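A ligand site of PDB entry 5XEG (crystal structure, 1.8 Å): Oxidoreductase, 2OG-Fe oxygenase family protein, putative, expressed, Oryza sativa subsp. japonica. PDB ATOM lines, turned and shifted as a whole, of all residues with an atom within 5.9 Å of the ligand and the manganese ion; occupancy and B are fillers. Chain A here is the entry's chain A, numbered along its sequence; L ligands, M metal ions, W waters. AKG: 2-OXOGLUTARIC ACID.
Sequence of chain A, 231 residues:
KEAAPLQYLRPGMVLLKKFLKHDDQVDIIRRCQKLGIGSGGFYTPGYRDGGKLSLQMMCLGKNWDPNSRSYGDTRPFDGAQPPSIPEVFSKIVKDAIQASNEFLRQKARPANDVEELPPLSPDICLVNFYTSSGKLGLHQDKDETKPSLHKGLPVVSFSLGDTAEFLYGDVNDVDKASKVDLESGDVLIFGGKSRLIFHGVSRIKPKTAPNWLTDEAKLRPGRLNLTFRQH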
ATOM      1  N   ARG A  48      16.209 -20.501 -17.853  1.00  0.00           N
ATOM      2  CA  ARG A  48      16.448 -19.108 -18.068  1.00  0.00           C
ATOM      3  C   ARG A  48      16.821 -18.482 -16.767  1.00  0.00           C
ATOM      4  O   ARG A  48      16.199 -18.792 -15.756  1.00  0.00           O
ATOM      5  CB  ARG A  48      15.202 -18.363 -18.598  1.00  0.00           C
ATOM      6  CG  ARG A  48      14.813 -18.705 -20.053  1.00  0.00           C
ATOM      7  CD  ARG A  48      15.838 -18.288 -21.122  1.00  0.00           C
ATOM      8  NE  ARG A  48      15.982 -16.861 -21.123  1.00  0.00           N
ATOM      9  CZ  ARG A  48      15.426 -15.976 -21.939  1.00  0.00           C
ATOM     10  NH1 ARG A  48      14.801 -16.316 -23.065  1.00  0.00           N
ATOM     11  NH2 ARG A  48      15.595 -14.712 -21.656  1.00  0.00           N
ATOM     12  N   TRP A  64      22.341 -18.076 -28.649  1.00  0.00           N
ATOM     13  CA  TRP A  64      22.576 -17.867 -27.220  1.00  0.00           C
ATOM     14  C   TRP A  64      22.090 -19.125 -26.463  1.00  0.00           C
ATOM     15  O   TRP A  64      20.886 -19.355 -26.338  1.00  0.00           O
ATOM     16  CB  TRP A  64      21.826 -16.630 -26.729  1.00  0.00           C
ATOM     17  CG  TRP A  64      21.908 -16.438 -25.246  1.00  0.00           C
ATOM     18  CD1 TRP A  64      23.033 -16.235 -24.495  1.00  0.00           C
ATOM     19  CD2 TRP A  64      20.813 -16.438 -24.314  1.00  0.00           C
ATOM     20  NE1 TRP A  64      22.709 -16.102 -23.171  1.00  0.00           N
ATOM     21  CE2 TRP A  64      21.354 -16.228 -23.032  1.00  0.00           C
ATOM     22  CE3 TRP A  64      19.429 -16.595 -24.452  1.00  0.00           C
ATOM     23  CZ2 TRP A  64      20.560 -16.167 -21.886  1.00  0.00           C
ATOM     24  CZ3 TRP A  64      18.646 -16.543 -23.317  1.00  0.00           C
ATOM     25  CH2 TRP A  64      19.205 -16.330 -22.048  1.00  0.00           C
ATOM     26  N   LEU A 126      17.426 -12.237 -29.764  1.00  0.00           N
ATOM     27  CA  LEU A 126      16.689 -13.262 -29.081  1.00  0.00           C
ATOM     28  C   LEU A 126      15.201 -12.934 -29.296  1.00  0.00           C
ATOM     29  O   LEU A 126      14.724 -11.816 -28.977  1.00  0.00           O
ATOM     30  CB  LEU A 126      17.029 -13.205 -27.624  1.00  0.00           C
ATOM     31  CG  LEU A 126      16.780 -14.365 -26.698  1.00  0.00           C
ATOM     32  CD1 LEU A 126      17.159 -13.905 -25.291  1.00  0.00           C
ATOM     33  CD2 LEU A 126      15.380 -14.930 -26.768  1.00  0.00           C
ATOM     34  N   ASN A 128      11.633 -14.080 -28.106  1.00  0.00           N
ATOM     35  CA  ASN A 128      10.902 -14.672 -27.015  1.00  0.00           C
ATOM     36  C   ASN A 128       9.417 -14.637 -27.357  1.00  0.00           C
ATOM     37  O   ASN A 128       8.873 -13.547 -27.675  1.00  0.00           O
ATOM     38  CB  ASN A 128      11.115 -13.823 -25.739  1.00  0.00           C
ATOM     39  CG  ASN A 128      12.504 -13.887 -25.197  1.00  0.00           C
ATOM     40  OD1 ASN A 128      12.984 -14.976 -24.830  1.00  0.00           O
ATOM     41  ND2 ASN A 128      13.170 -12.750 -25.108  1.00  0.00           N
ATOM     42  N   TYR A 130       5.800 -15.354 -25.466  1.00  0.00           N
ATOM     43  CA  TYR A 130       5.086 -15.651 -24.250  1.00  0.00           C
ATOM     44  C   TYR A 130       3.618 -15.896 -24.561  1.00  0.00           C
ATOM     45  O   TYR A 130       3.029 -15.072 -25.265  1.00  0.00           O
ATOM     46  CB  TYR A 130       5.127 -14.428 -23.347  1.00  0.00           C
ATOM     47  CG  TYR A 130       6.458 -13.908 -22.927  1.00  0.00           C
ATOM     48  CD1 TYR A 130       7.205 -13.095 -23.796  1.00  0.00           C
ATOM     49  CD2 TYR A 130       6.960 -14.155 -21.651  1.00  0.00           C
ATOM     50  CE1 TYR A 130       8.443 -12.587 -23.453  1.00  0.00           C
ATOM     51  CE2 TYR A 130       8.232 -13.661 -21.302  1.00  0.00           C
ATOM     52  CZ  TYR A 130       8.911 -12.832 -22.193  1.00  0.00           C
ATOM     53  OH  TYR A 130      10.131 -12.374 -21.762  1.00  0.00           O
ATOM     54  N   LEU A 136       8.967 -13.900 -17.069  1.00  0.00           N
ATOM     55  CA  LEU A 136      10.447 -14.052 -17.141  1.00  0.00           C
ATOM     56  C   LEU A 136      11.000 -13.313 -15.936  1.00  0.00           C
ATOM     57  O   LEU A 136      10.727 -12.124 -15.795  1.00  0.00           O
ATOM     58  CB  LEU A 136      11.016 -13.471 -18.421  1.00  0.00           C
ATOM     59  CG  LEU A 136      12.538 -13.621 -18.611  1.00  0.00           C
ATOM     60  CD1 LEU A 136      13.026 -15.051 -18.530  1.00  0.00           C
ATOM     61  CD2 LEU A 136      13.005 -12.927 -19.875  1.00  0.00           C
ATOM     62  N   HIS A 139      16.664 -10.608 -14.170  1.00  0.00           N
ATOM     63  CA  HIS A 139      18.016 -11.025 -14.506  1.00  0.00           C
ATOM     64  C   HIS A 139      18.719  -9.841 -15.156  1.00  0.00           C
ATOM     65  O   HIS A 139      18.054  -8.885 -15.607  1.00  0.00           O
ATOM     66  CB  HIS A 139      18.021 -12.215 -15.531  1.00  0.00           C
ATOM     67  CG  HIS A 139      17.390 -11.840 -16.819  1.00  0.00           C
ATOM     68  ND1 HIS A 139      16.026 -11.707 -16.944  1.00  0.00           N
ATOM     69  CD2 HIS A 139      17.918 -11.445 -17.995  1.00  0.00           C
ATOM     70  CE1 HIS A 139      15.746 -11.269 -18.158  1.00  0.00           C
ATOM     71  NE2 HIS A 139      16.874 -11.073 -18.787  1.00  0.00           N
ATOM     72  N   GLN A 140      20.039  -9.956 -15.279  1.00  0.00           N
ATOM     73  CA  GLN A 140      20.874  -9.028 -16.039  1.00  0.00           C
ATOM     74  C   GLN A 140      21.221  -9.718 -17.360  1.00  0.00           C
ATOM     75  O   GLN A 140      21.441 -10.900 -17.373  1.00  0.00           O
ATOM     76  CB  GLN A 140      22.184  -8.809 -15.277  1.00  0.00           C
ATOM     77  CG  GLN A 140      21.963  -7.964 -14.018  1.00  0.00           C
ATOM     78  CD  GLN A 140      23.259  -7.767 -13.231  1.00  0.00           C
ATOM     79  OE1 GLN A 140      23.949  -8.742 -12.844  1.00  0.00           O
ATOM     80  NE2 GLN A 140      23.619  -6.498 -12.977  1.00  0.00           N
ATOM     81  N   ASP A 141      21.399  -8.936 -18.407  1.00  0.00           N
ATOM     82  CA  ASP A 141      21.971  -9.365 -19.691  1.00  0.00           C
ATOM     83  C   ASP A 141      23.470  -9.233 -19.507  1.00  0.00           C
ATOM     84  O   ASP A 141      24.081  -8.242 -19.803  1.00  0.00           O
ATOM     85  CB  ASP A 141      21.458  -8.521 -20.855  1.00  0.00           C
ATOM     86  CG  ASP A 141      19.984  -8.831 -21.210  1.00  0.00           C
ATOM     87  OD1 ASP A 141      19.296  -9.633 -20.543  1.00  0.00           O
ATOM     88  OD2 ASP A 141      19.552  -8.257 -22.190  1.00  0.00           O
ATOM     89  N   SER A 157      15.009  -3.552 -27.513  1.00  0.00           N
ATOM     90  CA  SER A 157      13.956  -4.556 -27.353  1.00  0.00           C
ATOM     91  C   SER A 157      12.655  -4.096 -28.043  1.00  0.00           C
ATOM     92  O   SER A 157      12.116  -3.020 -27.711  1.00  0.00           O
ATOM     93  CB  SER A 157      13.664  -4.745 -25.884  1.00  0.00           C
ATOM     94  OG  SER A 157      12.459  -5.465 -25.575  1.00  0.00           O
ATOM     95  N   PHE A 158      12.163  -4.937 -28.934  1.00  0.00           N
ATOM     96  CA  PHE A 158      10.915  -4.712 -29.632  1.00  0.00           C
ATOM     97  C   PHE A 158       9.822  -5.465 -28.859  1.00  0.00           C
ATOM     98  O   PHE A 158      10.014  -6.622 -28.504  1.00  0.00           O
ATOM     99  CB  PHE A 158      10.850  -5.275 -31.055  1.00  0.00           C
ATOM    100  CG  PHE A 158      11.852  -4.715 -32.041  1.00  0.00           C
ATOM    101  CD1 PHE A 158      12.644  -3.634 -31.753  1.00  0.00           C
ATOM    102  CD2 PHE A 158      11.835  -5.210 -33.346  1.00  0.00           C
ATOM    103  CE1 PHE A 158      13.533  -3.144 -32.686  1.00  0.00           C
ATOM    104  CE2 PHE A 158      12.691  -4.688 -34.317  1.00  0.00           C
ATOM    105  CZ  PHE A 158      13.528  -3.648 -33.992  1.00  0.00           C
ATOM    106  N   SER A 159       8.626  -4.860 -28.796  1.00  0.00           N
ATOM    107  CA  SER A 159       7.468  -5.513 -28.184  1.00  0.00           C
ATOM    108  C   SER A 159       6.321  -5.573 -29.218  1.00  0.00           C
ATOM    109  O   SER A 159       6.003  -4.560 -29.876  1.00  0.00           O
ATOM    110  CB  SER A 159       6.982  -4.763 -26.950  1.00  0.00           C
ATOM    111  OG  SER A 159       7.864  -4.954 -25.805  1.00  0.00           O
ATOM    112  N   ALA A 164       3.216  -6.289 -22.036  1.00  0.00           N
ATOM    113  CA  ALA A 164       3.904  -6.864 -20.881  1.00  0.00           C
ATOM    114  C   ALA A 164       4.048  -5.833 -19.753  1.00  0.00           C
ATOM    115  O   ALA A 164       4.276  -4.650 -20.029  1.00  0.00           O
ATOM    116  CB  ALA A 164       5.298  -7.297 -21.293  1.00  0.00           C
ATOM    117  N   PHE A 166       6.736  -4.868 -17.451  1.00  0.00           N
ATOM    118  CA  PHE A 166       8.184  -5.063 -17.454  1.00  0.00           C
ATOM    119  C   PHE A 166       8.763  -4.469 -16.190  1.00  0.00           C
ATOM    120  O   PHE A 166       8.536  -3.271 -15.884  1.00  0.00           O
ATOM    121  CB  PHE A 166       8.747  -4.369 -18.702  1.00  0.00           C
ATOM    122  CG  PHE A 166      10.210  -4.491 -18.907  1.00  0.00           C
ATOM    123  CD1 PHE A 166      10.744  -5.643 -19.485  1.00  0.00           C
ATOM    124  CD2 PHE A 166      11.067  -3.446 -18.574  1.00  0.00           C
ATOM    125  CE1 PHE A 166      12.117  -5.743 -19.709  1.00  0.00           C
ATOM    126  CE2 PHE A 166      12.427  -3.567 -18.784  1.00  0.00           C
ATOM    127  CZ  PHE A 166      12.937  -4.665 -19.384  1.00  0.00           C
ATOM    128  N   LEU A 182       5.053  -2.346 -21.527  1.00  0.00           N
ATOM    129  CA  LEU A 182       5.544  -2.418 -22.891  1.00  0.00           C
ATOM    130  C   LEU A 182       4.418  -2.901 -23.719  1.00  0.00           C
ATOM    131  O   LEU A 182       3.964  -4.045 -23.585  1.00  0.00           O
ATOM    132  CB  LEU A 182       6.752  -3.329 -22.981  1.00  0.00           C
ATOM    133  CG  LEU A 182       7.937  -2.882 -22.088  1.00  0.00           C
ATOM    134  CD1 LEU A 182       9.084  -3.910 -22.239  1.00  0.00           C
ATOM    135  CD2 LEU A 182       8.454  -1.526 -22.472  1.00  0.00           C
ATOM    136  N   PHE A 190      18.130  -0.006 -23.314  1.00  0.00           N
ATOM    137  CA  PHE A 190      18.918   0.216 -22.140  1.00  0.00           C
ATOM    138  C   PHE A 190      20.386   0.006 -22.480  1.00  0.00           C
ATOM    139  O   PHE A 190      20.814  -1.068 -22.928  1.00  0.00           O
ATOM    140  CB  PHE A 190      18.456  -0.581 -20.899  1.00  0.00           C
ATOM    141  CG  PHE A 190      18.206  -2.050 -21.091  1.00  0.00           C
ATOM    142  CD1 PHE A 190      16.961  -2.514 -21.548  1.00  0.00           C
ATOM    143  CD2 PHE A 190      19.093  -3.022 -20.622  1.00  0.00           C
ATOM    144  CE1 PHE A 190      16.668  -3.855 -21.665  1.00  0.00           C
ATOM    145  CE2 PHE A 190      18.759  -4.408 -20.667  1.00  0.00           C
ATOM    146  CZ  PHE A 190      17.564  -4.798 -21.239  1.00  0.00           C
ATOM    147  N   HIS A 199      16.065  -6.989 -14.878  1.00  0.00           N
ATOM    148  CA  HIS A 199      14.837  -6.731 -15.602  1.00  0.00           C
ATOM    149  C   HIS A 199      14.132  -8.039 -15.873  1.00  0.00           C
ATOM    150  O   HIS A 199      14.717  -9.142 -15.764  1.00  0.00           O
ATOM    151  CB  HIS A 199      15.056  -5.955 -16.907  1.00  0.00           C
ATOM    152  CG  HIS A 199      15.951  -6.659 -17.851  1.00  0.00           C
ATOM    153  ND1 HIS A 199      17.331  -6.674 -17.687  1.00  0.00           N
ATOM    154  CD2 HIS A 199      15.684  -7.465 -18.899  1.00  0.00           C
ATOM    155  CE1 HIS A 199      17.861  -7.449 -18.612  1.00  0.00           C
ATOM    156  NE2 HIS A 199      16.898  -7.887 -19.397  1.00  0.00           N
ATOM    157  N   GLY A 200      12.840  -7.920 -16.140  1.00  0.00           N
ATOM    158  CA  GLY A 200      12.090  -9.125 -16.434  1.00  0.00           C
ATOM    159  C   GLY A 200      10.617  -8.790 -16.743  1.00  0.00           C
ATOM    160  O   GLY A 200      10.263  -7.629 -16.821  1.00  0.00           O
ATOM    161  N   VAL A 201       9.806  -9.819 -16.962  1.00  0.00           N
ATOM    162  CA  VAL A 201       8.409  -9.658 -17.379  1.00  0.00           C
ATOM    163  C   VAL A 201       7.552 -10.336 -16.272  1.00  0.00           C
ATOM    164  O   VAL A 201       7.645 -11.542 -16.082  1.00  0.00           O
ATOM    165  CB  VAL A 201       8.164 -10.275 -18.771  1.00  0.00           C
ATOM    166  CG1 VAL A 201       6.670 -10.219 -19.084  1.00  0.00           C
ATOM    167  CG2 VAL A 201       8.912  -9.524 -19.828  1.00  0.00           C
ATOM    168  N   ARG A 223       2.479 -12.515 -26.519  1.00  0.00           N
ATOM    169  CA  ARG A 223       3.389 -11.413 -26.807  1.00  0.00           C
ATOM    170  C   ARG A 223       4.677 -11.922 -27.460  1.00  0.00           C
ATOM    171  O   ARG A 223       5.227 -12.932 -27.019  1.00  0.00           O
ATOM    172  CB  ARG A 223       3.781 -10.693 -25.537  1.00  0.00           C
ATOM    173  CG  ARG A 223       4.814  -9.612 -25.730  1.00  0.00           C
ATOM    174  CD  ARG A 223       5.015  -8.847 -24.435  1.00  0.00           C
ATOM    175  NE  ARG A 223       6.157  -7.922 -24.520  1.00  0.00           N
ATOM    176  CZ  ARG A 223       7.422  -8.172 -24.127  1.00  0.00           C
ATOM    177  NH1 ARG A 223       7.800  -9.332 -23.586  1.00  0.00           N
ATOM    178  NH2 ARG A 223       8.336  -7.234 -24.270  1.00  0.00           N
ATOM    179  N   ASN A 225       8.525 -10.770 -28.256  1.00  0.00           N
ATOM    180  CA  ASN A 225       9.580  -9.832 -27.974  1.00  0.00           C
ATOM    181  C   ASN A 225      10.775 -10.197 -28.839  1.00  0.00           C
ATOM    182  O   ASN A 225      11.035 -11.382 -29.049  1.00  0.00           O
ATOM    183  CB  ASN A 225       9.984  -9.934 -26.493  1.00  0.00           C
ATOM    184  CG  ASN A 225      11.348  -9.323 -26.208  1.00  0.00           C
ATOM    185  OD1 ASN A 225      12.347 -10.016 -26.062  1.00  0.00           O
ATOM    186  ND2 ASN A 225      11.397  -8.004 -26.165  1.00  0.00           N
ATOM    187  N   THR A 227      14.847  -9.156 -28.765  1.00  0.00           N
ATOM    188  CA  THR A 227      15.834  -8.458 -27.976  1.00  0.00           C
ATOM    189  C   THR A 227      17.169  -8.544 -28.733  1.00  0.00           C
ATOM    190  O   THR A 227      17.649  -9.646 -28.953  1.00  0.00           O
ATOM    191  CB  THR A 227      15.938  -9.063 -26.580  1.00  0.00           C
ATOM    192  OG1 THR A 227      14.715  -8.714 -25.903  1.00  0.00           O
ATOM    193  CG2 THR A 227      17.117  -8.453 -25.852  1.00  0.00           C
ATOM    194  N   ARG A 229      21.261  -7.462 -29.254  1.00  0.00           N
ATOM    195  CA  ARG A 229      22.472  -7.142 -28.536  1.00  0.00           C
ATOM    196  C   ARG A 229      23.707  -7.329 -29.452  1.00  0.00           C
ATOM    197  O   ARG A 229      23.569  -7.906 -30.519  1.00  0.00           O
ATOM    198  CB  ARG A 229      22.618  -8.076 -27.322  1.00  0.00           C
ATOM    199  CG  ARG A 229      21.396  -8.060 -26.393  1.00  0.00           C
ATOM    200  CD  ARG A 229      21.657  -8.646 -25.022  1.00  0.00           C
ATOM    201  NE  ARG A 229      21.639 -10.081 -25.079  1.00  0.00           N
ATOM    202  CZ  ARG A 229      20.669 -10.901 -24.644  1.00  0.00           C
ATOM    203  NH1 ARG A 229      19.555 -10.506 -24.067  1.00  0.00           N
ATOM    204  NH2 ARG A 229      20.862 -12.190 -24.816  1.00  0.00           N
HETATM  205  C1  AKG L   1      15.479 -11.457 -22.352  1.00  0.00           C
HETATM  206  O1  AKG L   1      16.701 -11.375 -22.093  1.00  0.00           O
HETATM  207  O2  AKG L   1      14.992 -12.443 -22.937  1.00  0.00           O
HETATM  208  C2  AKG L   1      14.591 -10.373 -21.939  1.00  0.00           C
HETATM  209  O5  AKG L   1      14.845  -9.716 -20.947  1.00  0.00           O
HETATM  210  C3  AKG L   1      13.358 -10.060 -22.758  1.00  0.00           C
HETATM  211  C4  AKG L   1      12.350  -9.321 -21.892  1.00  0.00           C
HETATM  212  C5  AKG L   1      11.092  -9.073 -22.692  1.00  0.00           C
HETATM  213  O3  AKG L   1      10.734  -7.889 -22.893  1.00  0.00           O
HETATM  214  O4  AKG L   1      10.452 -10.050 -23.123  1.00  0.00           O
HETATM  215 MN    MN M   1      17.115  -9.720 -20.621  1.00  0.00          MN
HETATM  216  O   HOH W   1      14.993  -7.206 -23.476  1.00  0.00           O
HETATM  217  O   HOH W   2      12.328  -5.840 -23.079  1.00  0.00           O
HETATM  218  O   HOH W   3      18.942 -13.096 -22.782  1.00  0.00           O
HETATM  219  O   HOH W   4      17.059  -8.465 -22.424  1.00  0.00           O
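ND2 of Asn 128 is in hydrogen-bond range of O2 of the ligand (2.9 Å).
The side-chain amide nitrogen (ND2) of Asn 225 is in hydrogen-bond range of an oxygen (O3) of the ligand, 3.3 Å away.
The guanidinium group (NH1) of Arg 223 is in salt-bridge range of an oxygen (O4) of the ligand, 2.8 Å away.
NH2 of Arg 48 is in salt-bridge range of O2 of the ligand.
The guanidinium group of Arg 229 lies close to an oxygen (O1) of the ligand (3.6 Å).
An oxygen (O4) of the ligand sits at hydrogen-bond distance from the side-chain hydroxyl (OH) of Tyr 130, at 2.7 Å.
O of Tyr 130 is in hydrogen-bond range of N of Arg 223.
N of Val 201 sits at hydrogen-bond distance from O of Leu 136, at 2.7 Å.
The guanidinium group of Arg 48 lies within hydrogen-bond range of the side-chain amide oxygen of Asn 128 (2.9 Å).
The side-chain hydroxyl (OG) of Ser 159 is in hydrogen-bond range of the guanidinium group (NH2) of Arg 223, at 2.8 Å.
OD1 of Asn 225 sits at hydrogen-bond distance from OG1 of Thr 227 (2.7 Å).
ND2 of Asn 225 is in hydrogen-bond range of O of Phe 158 (3.0 Å).
The guanidinium group (NH1) of Arg 229 lies within salt-bridge range of the side-chain carboxylate (OD2) of Asp 141 (2.9 Å).
The side-chain amide nitrogen (ND2) of Asn 225 lies within hydrogen-bond range of the side-chain hydroxyl (OG) of Ser 157.
Residues that only touch the ligand: Leu 126, Val 201, Leu 136 and Thr 227.
Hydrophobic or aromatic side chains within 4 Å of the ligand: Leu 126, Tyr 130, Leu 136, His 139, His 199 and Val 201.
Within 4 Å of the ligand: Arg 48, Leu 126, Asn 128, Tyr 130, Leu 136, His 139, Asp 141, His 199, Val 201, Arg 223, Asn 225, Thr 227 and Arg 229.
Three residues have an atom within 4 Å of the manganese ion: His 139, Asp 141 and His 199.
The side-chain carboxylate (OD1) of Asp 141 is bound to the manganese ion, 2.2 Å away.
The manganese ion is bound by water W4, 2.2 Å away.
A ring nitrogen (NE2) of His 199 binds the manganese ion.
An oxygen (O1) of the ligand is bound to the manganese ion (2.3 Å).
NE2 of His 139 is bound to the manganese ion (2.3 Å).
An oxygen (O5) of the ligand binds the manganese ion, at 2.3 Å.
Water W2 bridges OG of Ser 157 (2.5 Å) and O3 of the ligand (2.6 Å).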
